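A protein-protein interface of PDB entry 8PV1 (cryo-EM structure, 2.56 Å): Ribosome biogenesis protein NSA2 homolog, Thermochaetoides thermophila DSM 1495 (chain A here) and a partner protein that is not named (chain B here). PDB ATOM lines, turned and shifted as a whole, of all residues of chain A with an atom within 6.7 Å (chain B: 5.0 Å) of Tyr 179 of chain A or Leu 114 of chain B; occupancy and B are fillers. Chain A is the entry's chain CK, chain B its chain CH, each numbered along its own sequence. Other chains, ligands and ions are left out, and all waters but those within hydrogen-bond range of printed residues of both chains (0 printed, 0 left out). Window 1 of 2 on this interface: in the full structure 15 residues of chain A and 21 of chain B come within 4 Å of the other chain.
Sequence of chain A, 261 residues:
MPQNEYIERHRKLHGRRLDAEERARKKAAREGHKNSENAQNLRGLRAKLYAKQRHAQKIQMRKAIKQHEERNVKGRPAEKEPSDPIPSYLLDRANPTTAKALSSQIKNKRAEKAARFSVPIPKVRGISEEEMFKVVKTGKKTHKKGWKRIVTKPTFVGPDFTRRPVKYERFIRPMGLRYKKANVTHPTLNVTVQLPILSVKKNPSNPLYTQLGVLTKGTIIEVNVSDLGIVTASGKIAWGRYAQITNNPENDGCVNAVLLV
The side-chain hydroxyl of Tyr 111 of chain B lies within hydrogen-bond range of the backbone carbonyl oxygen of Asp 252 of chain A (2.7 Å).
The backbone NH (N) of Thr 155 of chain A is in hydrogen-bond range of the backbone carbonyl oxygen (O) of Leu 177 of chain A, at 3.1 Å.
The side-chain hydroxyl of Tyr 179 of chain A is in hydrogen-bond range of the backbone carbonyl oxygen of Gly 253 of chain A, 3.0 Å away.
The side-chain carboxylate (OD1) of Asp 110 of chain B is in salt-bridge range of the guanidinium group (NH1) of Arg 113 of chain B (3.2 Å).
O of Thr 155 of chain A sits at hydrogen-bond distance from N of Tyr 179 of chain A (3.0 Å).
Among the printed residues, pairs that only touch across the chains: Gly 176 of chain A with Arg 113 of chain B (3.7 Å), Gly 176 of chain A with Leu 114 of chain B (3.7 Å), Gly 253 of chain A with Leu 114 of chain B (3.7 Å), Leu 177 of chain A with Leu 114 of chain B (3.8 Å), Glu 250 of chain A with Leu 127 of chain B (3.9 Å), Leu 177 of chain A with Tyr 117 of chain B (3.9 Å), Tyr 179 of chain A with Leu 114 of chain B (3.9 Å) and Gly 253 of chain A with Tyr 111 of chain B (3.99 Å).
Tyr 179 of chain A touches just one residue of chain B: Leu 114.
Leu 114 of chain B touches four residues of chain A.
Printed residues of chain B within 4 Å of Gly 253 of chain A: Tyr 111 and Leu 114.
Of the printed residues of chain B, Asp 252 of chain A touches Tyr 111.
Val 112 of chain B touches none of the printed residues of chain A.
Val 255 of chain A touches none of the printed residues of chain B.
The nearest printed residue of chain B that does not touch Tyr 179 of chain A is Leu 127 of chain B (6.6 Å).
The nearest residue of chain A that does not touch Leu 114 of chain B is Asp 252 of chain A (5.5 Å).
Printed residues of chain B that touch a printed residue of chain A: Tyr 111, Arg 113, Leu 114, Tyr 117 and Leu 127.
Printed residues of chain A that touch a printed residue of chain B: Gly 176, Leu 177, Tyr 179, Glu 250, Asp 252 and Gly 253.
Hydrophobic or aromatic side chains of chain A within 4 Å of the printed part of chain B: Leu 177 and Tyr 179.
Among the printed residues, 9 pairs touch across the chains.
Among the printed residues, no Asp or Glu carboxylate lies within 4 Å of a Lys or Arg side-chain nitrogen of the other chain.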
ATOM      1  N   PRO A 154       5.807  19.475  12.316  1.00  0.00           N
ATOM      2  CA  PRO A 154       4.665  19.102  11.470  1.00  0.00           C
ATOM      3  C   PRO A 154       5.069  18.270  10.261  1.00  0.00           C
ATOM      4  O   PRO A 154       6.137  18.460   9.678  1.00  0.00           O
ATOM      5  CB  PRO A 154       4.089  20.456  11.044  1.00  0.00           C
ATOM      6  CG  PRO A 154       4.478  21.370  12.121  1.00  0.00           C
ATOM      7  CD  PRO A 154       5.835  20.930  12.556  1.00  0.00           C
ATOM      8  N   THR A 155       4.195  17.334   9.888  1.00  0.00           N
ATOM      9  CA  THR A 155       4.452  16.423   8.783  1.00  0.00           C
ATOM     10  C   THR A 155       3.263  16.377   7.836  1.00  0.00           C
ATOM     11  O   THR A 155       2.156  16.814   8.161  1.00  0.00           O
ATOM     12  CB  THR A 155       4.756  14.990   9.249  1.00  0.00           C
ATOM     13  OG1 THR A 155       3.646  14.476   9.995  1.00  0.00           O
ATOM     14  CG2 THR A 155       6.015  14.938  10.082  1.00  0.00           C
ATOM     15  N   PHE A 156       3.523  15.840   6.648  1.00  0.00           N
ATOM     16  CA  PHE A 156       2.507  15.531   5.651  1.00  0.00           C
ATOM     17  C   PHE A 156       2.595  14.038   5.365  1.00  0.00           C
ATOM     18  O   PHE A 156       3.641  13.553   4.924  1.00  0.00           O
ATOM     19  CB  PHE A 156       2.725  16.361   4.382  1.00  0.00           C
ATOM     20  CG  PHE A 156       1.849  15.965   3.231  1.00  0.00           C
ATOM     21  CD1 PHE A 156       0.552  16.438   3.145  1.00  0.00           C
ATOM     22  CD2 PHE A 156       2.326  15.144   2.221  1.00  0.00           C
ATOM     23  CE1 PHE A 156      -0.256  16.086   2.091  1.00  0.00           C
ATOM     24  CE2 PHE A 156       1.520  14.787   1.167  1.00  0.00           C
ATOM     25  CZ  PHE A 156       0.228  15.260   1.100  1.00  0.00           C
ATOM     26  N   VAL A 157       1.504  13.311   5.619  1.00  0.00           N
ATOM     27  CA  VAL A 157       1.528  11.853   5.527  1.00  0.00           C
ATOM     28  C   VAL A 157       0.969  11.320   4.214  1.00  0.00           C
ATOM     29  O   VAL A 157       1.094  10.114   3.949  1.00  0.00           O
ATOM     30  CB  VAL A 157       0.778  11.202   6.709  1.00  0.00           C
ATOM     31  CG1 VAL A 157       1.396  11.627   8.026  1.00  0.00           C
ATOM     32  CG2 VAL A 157      -0.702  11.548   6.661  1.00  0.00           C
ATOM     33  N   GLY A 158       0.355  12.164   3.392  1.00  0.00           N
ATOM     34  CA  GLY A 158      -0.136  11.741   2.102  1.00  0.00           C
ATOM     35  C   GLY A 158      -1.514  11.112   2.154  1.00  0.00           C
ATOM     36  O   GLY A 158      -2.077  10.875   3.227  1.00  0.00           O
ATOM     37  N   MET A 175      -1.035  12.610  15.072  1.00  0.00           N
ATOM     38  CA  MET A 175      -2.129  13.099  14.237  1.00  0.00           C
ATOM     39  C   MET A 175      -2.334  14.599  14.390  1.00  0.00           C
ATOM     40  O   MET A 175      -2.729  15.280  13.439  1.00  0.00           O
ATOM     41  CB  MET A 175      -3.418  12.356  14.581  1.00  0.00           C
ATOM     42  CG  MET A 175      -3.332  10.853  14.426  1.00  0.00           C
ATOM     43  SD  MET A 175      -4.952  10.068  14.498  1.00  0.00           S
ATOM     44  CE  MET A 175      -5.121   9.831  16.261  1.00  0.00           C
ATOM     45  N   GLY A 176      -2.067  15.133  15.581  1.00  0.00           N
ATOM     46  CA  GLY A 176      -2.260  16.549  15.822  1.00  0.00           C
ATOM     47  C   GLY A 176      -1.241  17.447  15.156  1.00  0.00           C
ATOM     48  O   GLY A 176      -1.442  18.664  15.128  1.00  0.00           O
ATOM     49  N   LEU A 177      -0.157  16.880  14.629  1.00  0.00           N
ATOM     50  CA  LEU A 177       0.857  17.634  13.909  1.00  0.00           C
ATOM     51  C   LEU A 177       0.808  17.398  12.405  1.00  0.00           C
ATOM     52  O   LEU A 177       1.707  17.845  11.691  1.00  0.00           O
ATOM     53  CB  LEU A 177       2.247  17.292  14.448  1.00  0.00           C
ATOM     54  CG  LEU A 177       2.677  17.991  15.739  1.00  0.00           C
ATOM     55  CD1 LEU A 177       3.900  17.316  16.327  1.00  0.00           C
ATOM     56  CD2 LEU A 177       2.956  19.457  15.486  1.00  0.00           C
ATOM     57  N   ARG A 178      -0.211  16.710  11.903  1.00  0.00           N
ATOM     58  CA  ARG A 178      -0.319  16.435  10.477  1.00  0.00           C
ATOM     59  C   ARG A 178      -1.042  17.580   9.782  1.00  0.00           C
ATOM     60  O   ARG A 178      -2.039  18.096  10.294  1.00  0.00           O
ATOM     61  CB  ARG A 178      -1.049  15.116  10.233  1.00  0.00           C
ATOM     62  CG  ARG A 178      -0.334  13.909  10.799  1.00  0.00           C
ATOM     63  CD  ARG A 178      -1.148  12.651  10.608  1.00  0.00           C
ATOM     64  NE  ARG A 178      -0.610  11.539  11.379  1.00  0.00           N
ATOM     65  CZ  ARG A 178      -1.173  10.343  11.459  1.00  0.00           C
ATOM     66  NH1 ARG A 178      -2.288  10.059  10.809  1.00  0.00           N
ATOM     67  NH2 ARG A 178      -0.603   9.407  12.211  1.00  0.00           N
ATOM     68  N   TYR A 179      -0.532  17.977   8.620  1.00  0.00           N
ATOM     69  CA  TYR A 179      -1.088  19.075   7.847  1.00  0.00           C
ATOM     70  C   TYR A 179      -1.393  18.615   6.430  1.00  0.00           C
ATOM     71  O   TYR A 179      -0.750  17.705   5.901  1.00  0.00           O
ATOM     72  CB  TYR A 179      -0.131  20.270   7.801  1.00  0.00           C
ATOM     73  CG  TYR A 179      -0.118  21.098   9.062  1.00  0.00           C
ATOM     74  CD1 TYR A 179       0.601  20.689  10.174  1.00  0.00           C
ATOM     75  CD2 TYR A 179      -0.827  22.288   9.141  1.00  0.00           C
ATOM     76  CE1 TYR A 179       0.614  21.439  11.329  1.00  0.00           C
ATOM     77  CE2 TYR A 179      -0.820  23.045  10.292  1.00  0.00           C
ATOM     78  CZ  TYR A 179      -0.096  22.617  11.384  1.00  0.00           C
ATOM     79  OH  TYR A 179      -0.083  23.366  12.536  1.00  0.00           O
ATOM     80  N   LYS A 180      -2.385  19.262   5.818  1.00  0.00           N
ATOM     81  CA  LYS A 180      -2.788  18.956   4.455  1.00  0.00           C
ATOM     82  C   LYS A 180      -2.836  20.165   3.538  1.00  0.00           C
ATOM     83  O   LYS A 180      -2.852  19.985   2.316  1.00  0.00           O
ATOM     84  CB  LYS A 180      -4.171  18.285   4.441  1.00  0.00           C
ATOM     85  CG  LYS A 180      -4.182  16.873   4.987  1.00  0.00           C
ATOM     86  CD  LYS A 180      -5.569  16.266   4.903  1.00  0.00           C
ATOM     87  CE  LYS A 180      -5.557  14.813   5.345  1.00  0.00           C
ATOM     88  NZ  LYS A 180      -6.911  14.200   5.296  1.00  0.00           N
ATOM     89  N   LYS A 181      -2.855  21.380   4.078  1.00  0.00           N
ATOM     90  CA  LYS A 181      -2.998  22.591   3.287  1.00  0.00           C
ATOM     91  C   LYS A 181      -1.932  23.600   3.692  1.00  0.00           C
ATOM     92  O   LYS A 181      -1.314  23.498   4.753  1.00  0.00           O
ATOM     93  CB  LYS A 181      -4.396  23.201   3.448  1.00  0.00           C
ATOM     94  CG  LYS A 181      -5.504  22.363   2.839  1.00  0.00           C
ATOM     95  CD  LYS A 181      -6.856  23.018   3.024  1.00  0.00           C
ATOM     96  CE  LYS A 181      -7.957  22.181   2.401  1.00  0.00           C
ATOM     97  NZ  LYS A 181      -7.837  22.138   0.919  1.00  0.00           N
ATOM     98  N   ILE A 197      -1.609  20.319  -0.121  1.00  0.00           N
ATOM     99  CA  ILE A 197      -0.245  19.836  -0.284  1.00  0.00           C
ATOM    100  C   ILE A 197      -0.296  18.518  -1.037  1.00  0.00           C
ATOM    101  O   ILE A 197      -1.060  17.616  -0.675  1.00  0.00           O
ATOM    102  CB  ILE A 197       0.451  19.669   1.077  1.00  0.00           C
ATOM    103  CG1 ILE A 197       0.462  20.991   1.842  1.00  0.00           C
ATOM    104  CG2 ILE A 197       1.868  19.145   0.897  1.00  0.00           C
ATOM    105  CD1 ILE A 197       1.071  20.886   3.214  1.00  0.00           C
ATOM    106  N   LEU A 215       7.585  19.173   7.529  1.00  0.00           N
ATOM    107  CA  LEU A 215       7.330  20.505   6.990  1.00  0.00           C
ATOM    108  C   LEU A 215       8.034  21.526   7.877  1.00  0.00           C
ATOM    109  O   LEU A 215       7.485  21.960   8.892  1.00  0.00           O
ATOM    110  CB  LEU A 215       5.832  20.783   6.919  1.00  0.00           C
ATOM    111  CG  LEU A 215       4.976  19.749   6.195  1.00  0.00           C
ATOM    112  CD1 LEU A 215       3.528  19.857   6.625  1.00  0.00           C
ATOM    113  CD2 LEU A 215       5.104  19.931   4.700  1.00  0.00           C
ATOM    114  N   PRO A 249       6.498  26.203  10.754  1.00  0.00           N
ATOM    115  CA  PRO A 249       5.168  25.702  11.133  1.00  0.00           C
ATOM    116  C   PRO A 249       5.085  25.183  12.555  1.00  0.00           C
ATOM    117  O   PRO A 249       4.012  25.267  13.166  1.00  0.00           O
ATOM    118  CB  PRO A 249       4.914  24.587  10.108  1.00  0.00           C
ATOM    119  CG  PRO A 249       5.830  24.900   8.967  1.00  0.00           C
ATOM    120  CD  PRO A 249       7.049  25.476   9.600  1.00  0.00           C
ATOM    121  N   GLU A 250       6.187  24.668  13.108  1.00  0.00           N
ATOM    122  CA  GLU A 250       6.172  24.178  14.483  1.00  0.00           C
ATOM    123  C   GLU A 250       5.978  25.311  15.482  1.00  0.00           C
ATOM    124  O   GLU A 250       5.493  25.080  16.594  1.00  0.00           O
ATOM    125  CB  GLU A 250       7.460  23.406  14.787  1.00  0.00           C
ATOM    126  CG  GLU A 250       8.715  24.259  14.933  1.00  0.00           C
ATOM    127  CD  GLU A 250       9.407  24.539  13.611  1.00  0.00           C
ATOM    128  OE1 GLU A 250       8.924  24.064  12.562  1.00  0.00           O
ATOM    129  OE2 GLU A 250      10.442  25.235  13.622  1.00  0.00           O
ATOM    130  N   ASP A 252       4.402  28.392  14.373  1.00  0.00           N
ATOM    131  CA  ASP A 252       3.291  29.226  13.936  1.00  0.00           C
ATOM    132  C   ASP A 252       1.948  28.509  13.909  1.00  0.00           C
ATOM    133  O   ASP A 252       0.912  29.179  13.961  1.00  0.00           O
ATOM    134  CB  ASP A 252       3.576  29.793  12.542  1.00  0.00           C
ATOM    135  CG  ASP A 252       4.720  30.779  12.546  1.00  0.00           C
ATOM    136  OD1 ASP A 252       5.430  30.876  11.525  1.00  0.00           O
ATOM    137  OD2 ASP A 252       4.914  31.453  13.577  1.00  0.00           O
ATOM    138  N   GLY A 253       1.930  27.182  13.823  1.00  0.00           N
ATOM    139  CA  GLY A 253       0.674  26.483  13.666  1.00  0.00           C
ATOM    140  C   GLY A 253       0.077  26.559  12.282  1.00  0.00           C
ATOM    141  O   GLY A 253      -1.080  26.163  12.101  1.00  0.00           O
ATOM    142  N   CYS A 254       0.824  27.061  11.302  1.00  0.00           N
ATOM    143  CA  CYS A 254       0.356  27.153   9.930  1.00  0.00           C
ATOM    144  C   CYS A 254       1.550  27.005   9.004  1.00  0.00           C
ATOM    145  O   CYS A 254       2.684  27.328   9.368  1.00  0.00           O
ATOM    146  CB  CYS A 254      -0.367  28.479   9.665  1.00  0.00           C
ATOM    147  SG  CYS A 254       0.630  29.954   9.988  1.00  0.00           S
ATOM    148  N   VAL A 255       1.286  26.514   7.799  1.00  0.00           N
ATOM    149  CA  VAL A 255       2.306  26.355   6.771  1.00  0.00           C
ATOM    150  C   VAL A 255       2.155  27.506   5.787  1.00  0.00           C
ATOM    151  O   VAL A 255       1.097  27.666   5.168  1.00  0.00           O
ATOM    152  CB  VAL A 255       2.190  25.000   6.058  1.00  0.00           C
ATOM    153  CG1 VAL A 255       3.294  24.848   5.027  1.00  0.00           C
ATOM    154  CG2 VAL A 255       2.235  23.864   7.067  1.00  0.00           C
ATOM    155  N   ASP B 110      -7.110  23.884  18.265  1.00  0.00           N
ATOM    156  CA  ASP B 110      -5.935  23.571  17.454  1.00  0.00           C
ATOM    157  C   ASP B 110      -4.641  23.896  18.192  1.00  0.00           C
ATOM    158  O   ASP B 110      -3.701  23.091  18.213  1.00  0.00           O
ATOM    159  CB  ASP B 110      -5.998  24.333  16.132  1.00  0.00           C
ATOM    160  CG  ASP B 110      -7.075  23.807  15.208  1.00  0.00           C
ATOM    161  OD1 ASP B 110      -7.562  22.682  15.445  1.00  0.00           O
ATOM    162  OD2 ASP B 110      -7.435  24.518  14.247  1.00  0.00           O
ATOM    163  N   TYR B 111      -4.580  25.065  18.832  1.00  0.00           N
ATOM    164  CA  TYR B 111      -3.333  25.439  19.487  1.00  0.00           C
ATOM    165  C   TYR B 111      -3.119  24.711  20.809  1.00  0.00           C
ATOM    166  O   TYR B 111      -1.970  24.504  21.203  1.00  0.00           O
ATOM    167  CB  TYR B 111      -3.262  26.952  19.663  1.00  0.00           C
ATOM    168  CG  TYR B 111      -2.836  27.639  18.388  1.00  0.00           C
ATOM    169  CD1 TYR B 111      -1.492  27.772  18.067  1.00  0.00           C
ATOM    170  CD2 TYR B 111      -3.773  28.126  17.492  1.00  0.00           C
ATOM    171  CE1 TYR B 111      -1.097  28.382  16.896  1.00  0.00           C
ATOM    172  CE2 TYR B 111      -3.388  28.742  16.321  1.00  0.00           C
ATOM    173  CZ  TYR B 111      -2.050  28.868  16.026  1.00  0.00           C
ATOM    174  OH  TYR B 111      -1.664  29.482  14.859  1.00  0.00           O
ATOM    175  N   VAL B 112      -4.188  24.286  21.489  1.00  0.00           N
ATOM    176  CA  VAL B 112      -4.022  23.402  22.641  1.00  0.00           C
ATOM    177  C   VAL B 112      -3.459  22.054  22.201  1.00  0.00           C
ATOM    178  O   VAL B 112      -2.554  21.497  22.847  1.00  0.00           O
ATOM    179  CB  VAL B 112      -5.358  23.260  23.397  1.00  0.00           C
ATOM    180  CG1 VAL B 112      -5.347  22.056  24.321  1.00  0.00           C
ATOM    181  CG2 VAL B 112      -5.628  24.512  24.210  1.00  0.00           C
ATOM    182  N   ARG B 113      -3.955  21.526  21.077  1.00  0.00           N
ATOM    183  CA  ARG B 113      -3.421  20.272  20.553  1.00  0.00           C
ATOM    184  C   ARG B 113      -1.954  20.407  20.154  1.00  0.00           C
ATOM    185  O   ARG B 113      -1.169  19.470  20.333  1.00  0.00           O
ATOM    186  CB  ARG B 113      -4.261  19.803  19.368  1.00  0.00           C
ATOM    187  CG  ARG B 113      -4.081  18.337  19.032  1.00  0.00           C
ATOM    188  CD  ARG B 113      -4.975  17.913  17.884  1.00  0.00           C
ATOM    189  NE  ARG B 113      -6.375  18.245  18.111  1.00  0.00           N
ATOM    190  CZ  ARG B 113      -7.062  19.122  17.393  1.00  0.00           C
ATOM    191  NH1 ARG B 113      -6.500  19.792  16.402  1.00  0.00           N
ATOM    192  NH2 ARG B 113      -8.343  19.332  17.677  1.00  0.00           N
ATOM    193  N   LEU B 114      -1.563  21.564  19.610  1.00  0.00           N
ATOM    194  CA  LEU B 114      -0.152  21.782  19.289  1.00  0.00           C
ATOM    195  C   LEU B 114       0.699  21.939  20.547  1.00  0.00           C
ATOM    196  O   LEU B 114       1.848  21.475  20.599  1.00  0.00           O
ATOM    197  CB  LEU B 114      -0.001  23.006  18.389  1.00  0.00           C
ATOM    198  CG  LEU B 114      -0.630  22.899  17.003  1.00  0.00           C
ATOM    199  CD1 LEU B 114      -0.623  24.248  16.322  1.00  0.00           C
ATOM    200  CD2 LEU B 114       0.093  21.863  16.164  1.00  0.00           C
ATOM    201  N   LEU B 115       0.154  22.603  21.572  1.00  0.00           N
ATOM    202  CA  LEU B 115       0.882  22.778  22.822  1.00  0.00           C
ATOM    203  C   LEU B 115       1.078  21.458  23.549  1.00  0.00           C
ATOM    204  O   LEU B 115       1.987  21.339  24.375  1.00  0.00           O
ATOM    205  CB  LEU B 115       0.152  23.773  23.722  1.00  0.00           C
ATOM    206  CG  LEU B 115       0.424  25.248  23.439  1.00  0.00           C
ATOM    207  CD1 LEU B 115      -0.494  26.127  24.262  1.00  0.00           C
ATOM    208  CD2 LEU B 115       1.878  25.577  23.714  1.00  0.00           C
ATOM    209  N   LYS B 116       0.229  20.463  23.271  1.00  0.00           N
ATOM    210  CA  LYS B 116       0.485  19.117  23.785  1.00  0.00           C
ATOM    211  C   LYS B 116       1.799  18.529  23.280  1.00  0.00           C
ATOM    212  O   LYS B 116       2.370  17.658  23.946  1.00  0.00           O
ATOM    213  CB  LYS B 116      -0.643  18.158  23.410  1.00  0.00           C
ATOM    214  CG  LYS B 116      -1.993  18.468  24.017  1.00  0.00           C
ATOM    215  CD  LYS B 116      -2.916  17.255  23.947  1.00  0.00           C
ATOM    216  CE  LYS B 116      -2.859  16.570  22.587  1.00  0.00           C
ATOM    217  NZ  LYS B 116      -3.554  15.258  22.594  1.00  0.00           N
ATOM    218  N   TYR B 117       2.287  18.972  22.124  1.00  0.00           N
ATOM    219  CA  TYR B 117       3.490  18.420  21.522  1.00  0.00           C
ATOM    220  C   TYR B 117       4.653  19.399  21.487  1.00  0.00           C
ATOM    221  O   TYR B 117       5.749  19.008  21.071  1.00  0.00           O
ATOM    222  CB  TYR B 117       3.191  17.934  20.099  1.00  0.00           C
ATOM    223  CG  TYR B 117       2.228  16.774  20.033  1.00  0.00           C
ATOM    224  CD1 TYR B 117       2.614  15.505  20.439  1.00  0.00           C
ATOM    225  CD2 TYR B 117       0.936  16.947  19.561  1.00  0.00           C
ATOM    226  CE1 TYR B 117       1.741  14.444  20.380  1.00  0.00           C
ATOM    227  CE2 TYR B 117       0.055  15.890  19.497  1.00  0.00           C
ATOM    228  CZ  TYR B 117       0.462  14.642  19.909  1.00  0.00           C
ATOM    229  OH  TYR B 117      -0.415  13.587  19.845  1.00  0.00           O
ATOM    230  N   ALA B 118       4.441  20.657  21.876  1.00  0.00           N
ATOM    231  CA  ALA B 118       5.535  21.625  21.904  1.00  0.00           C
ATOM    232  C   ALA B 118       6.627  21.195  22.884  1.00  0.00           C
ATOM    233  O   ALA B 118       6.357  20.611  23.936  1.00  0.00           O
ATOM    234  CB  ALA B 118       5.011  23.009  22.274  1.00  0.00           C
ATOM    235  N   LEU B 127       3.587  29.599  20.036  1.00  0.00           N
ATOM    236  CA  LEU B 127       2.250  29.064  19.784  1.00  0.00           C
ATOM    237  C   LEU B 127       1.176  29.844  20.536  1.00  0.00           C
ATOM    238  O   LEU B 127       0.091  30.098  19.993  1.00  0.00           O
ATOM    239  CB  LEU B 127       2.203  27.585  20.159  1.00  0.00           C
ATOM    240  CG  LEU B 127       2.899  26.638  19.182  1.00  0.00           C
ATOM    241  CD1 LEU B 127       3.015  25.250  19.778  1.00  0.00           C
ATOM    242  CD2 LEU B 127       2.153  26.599  17.862  1.00  0.00           C
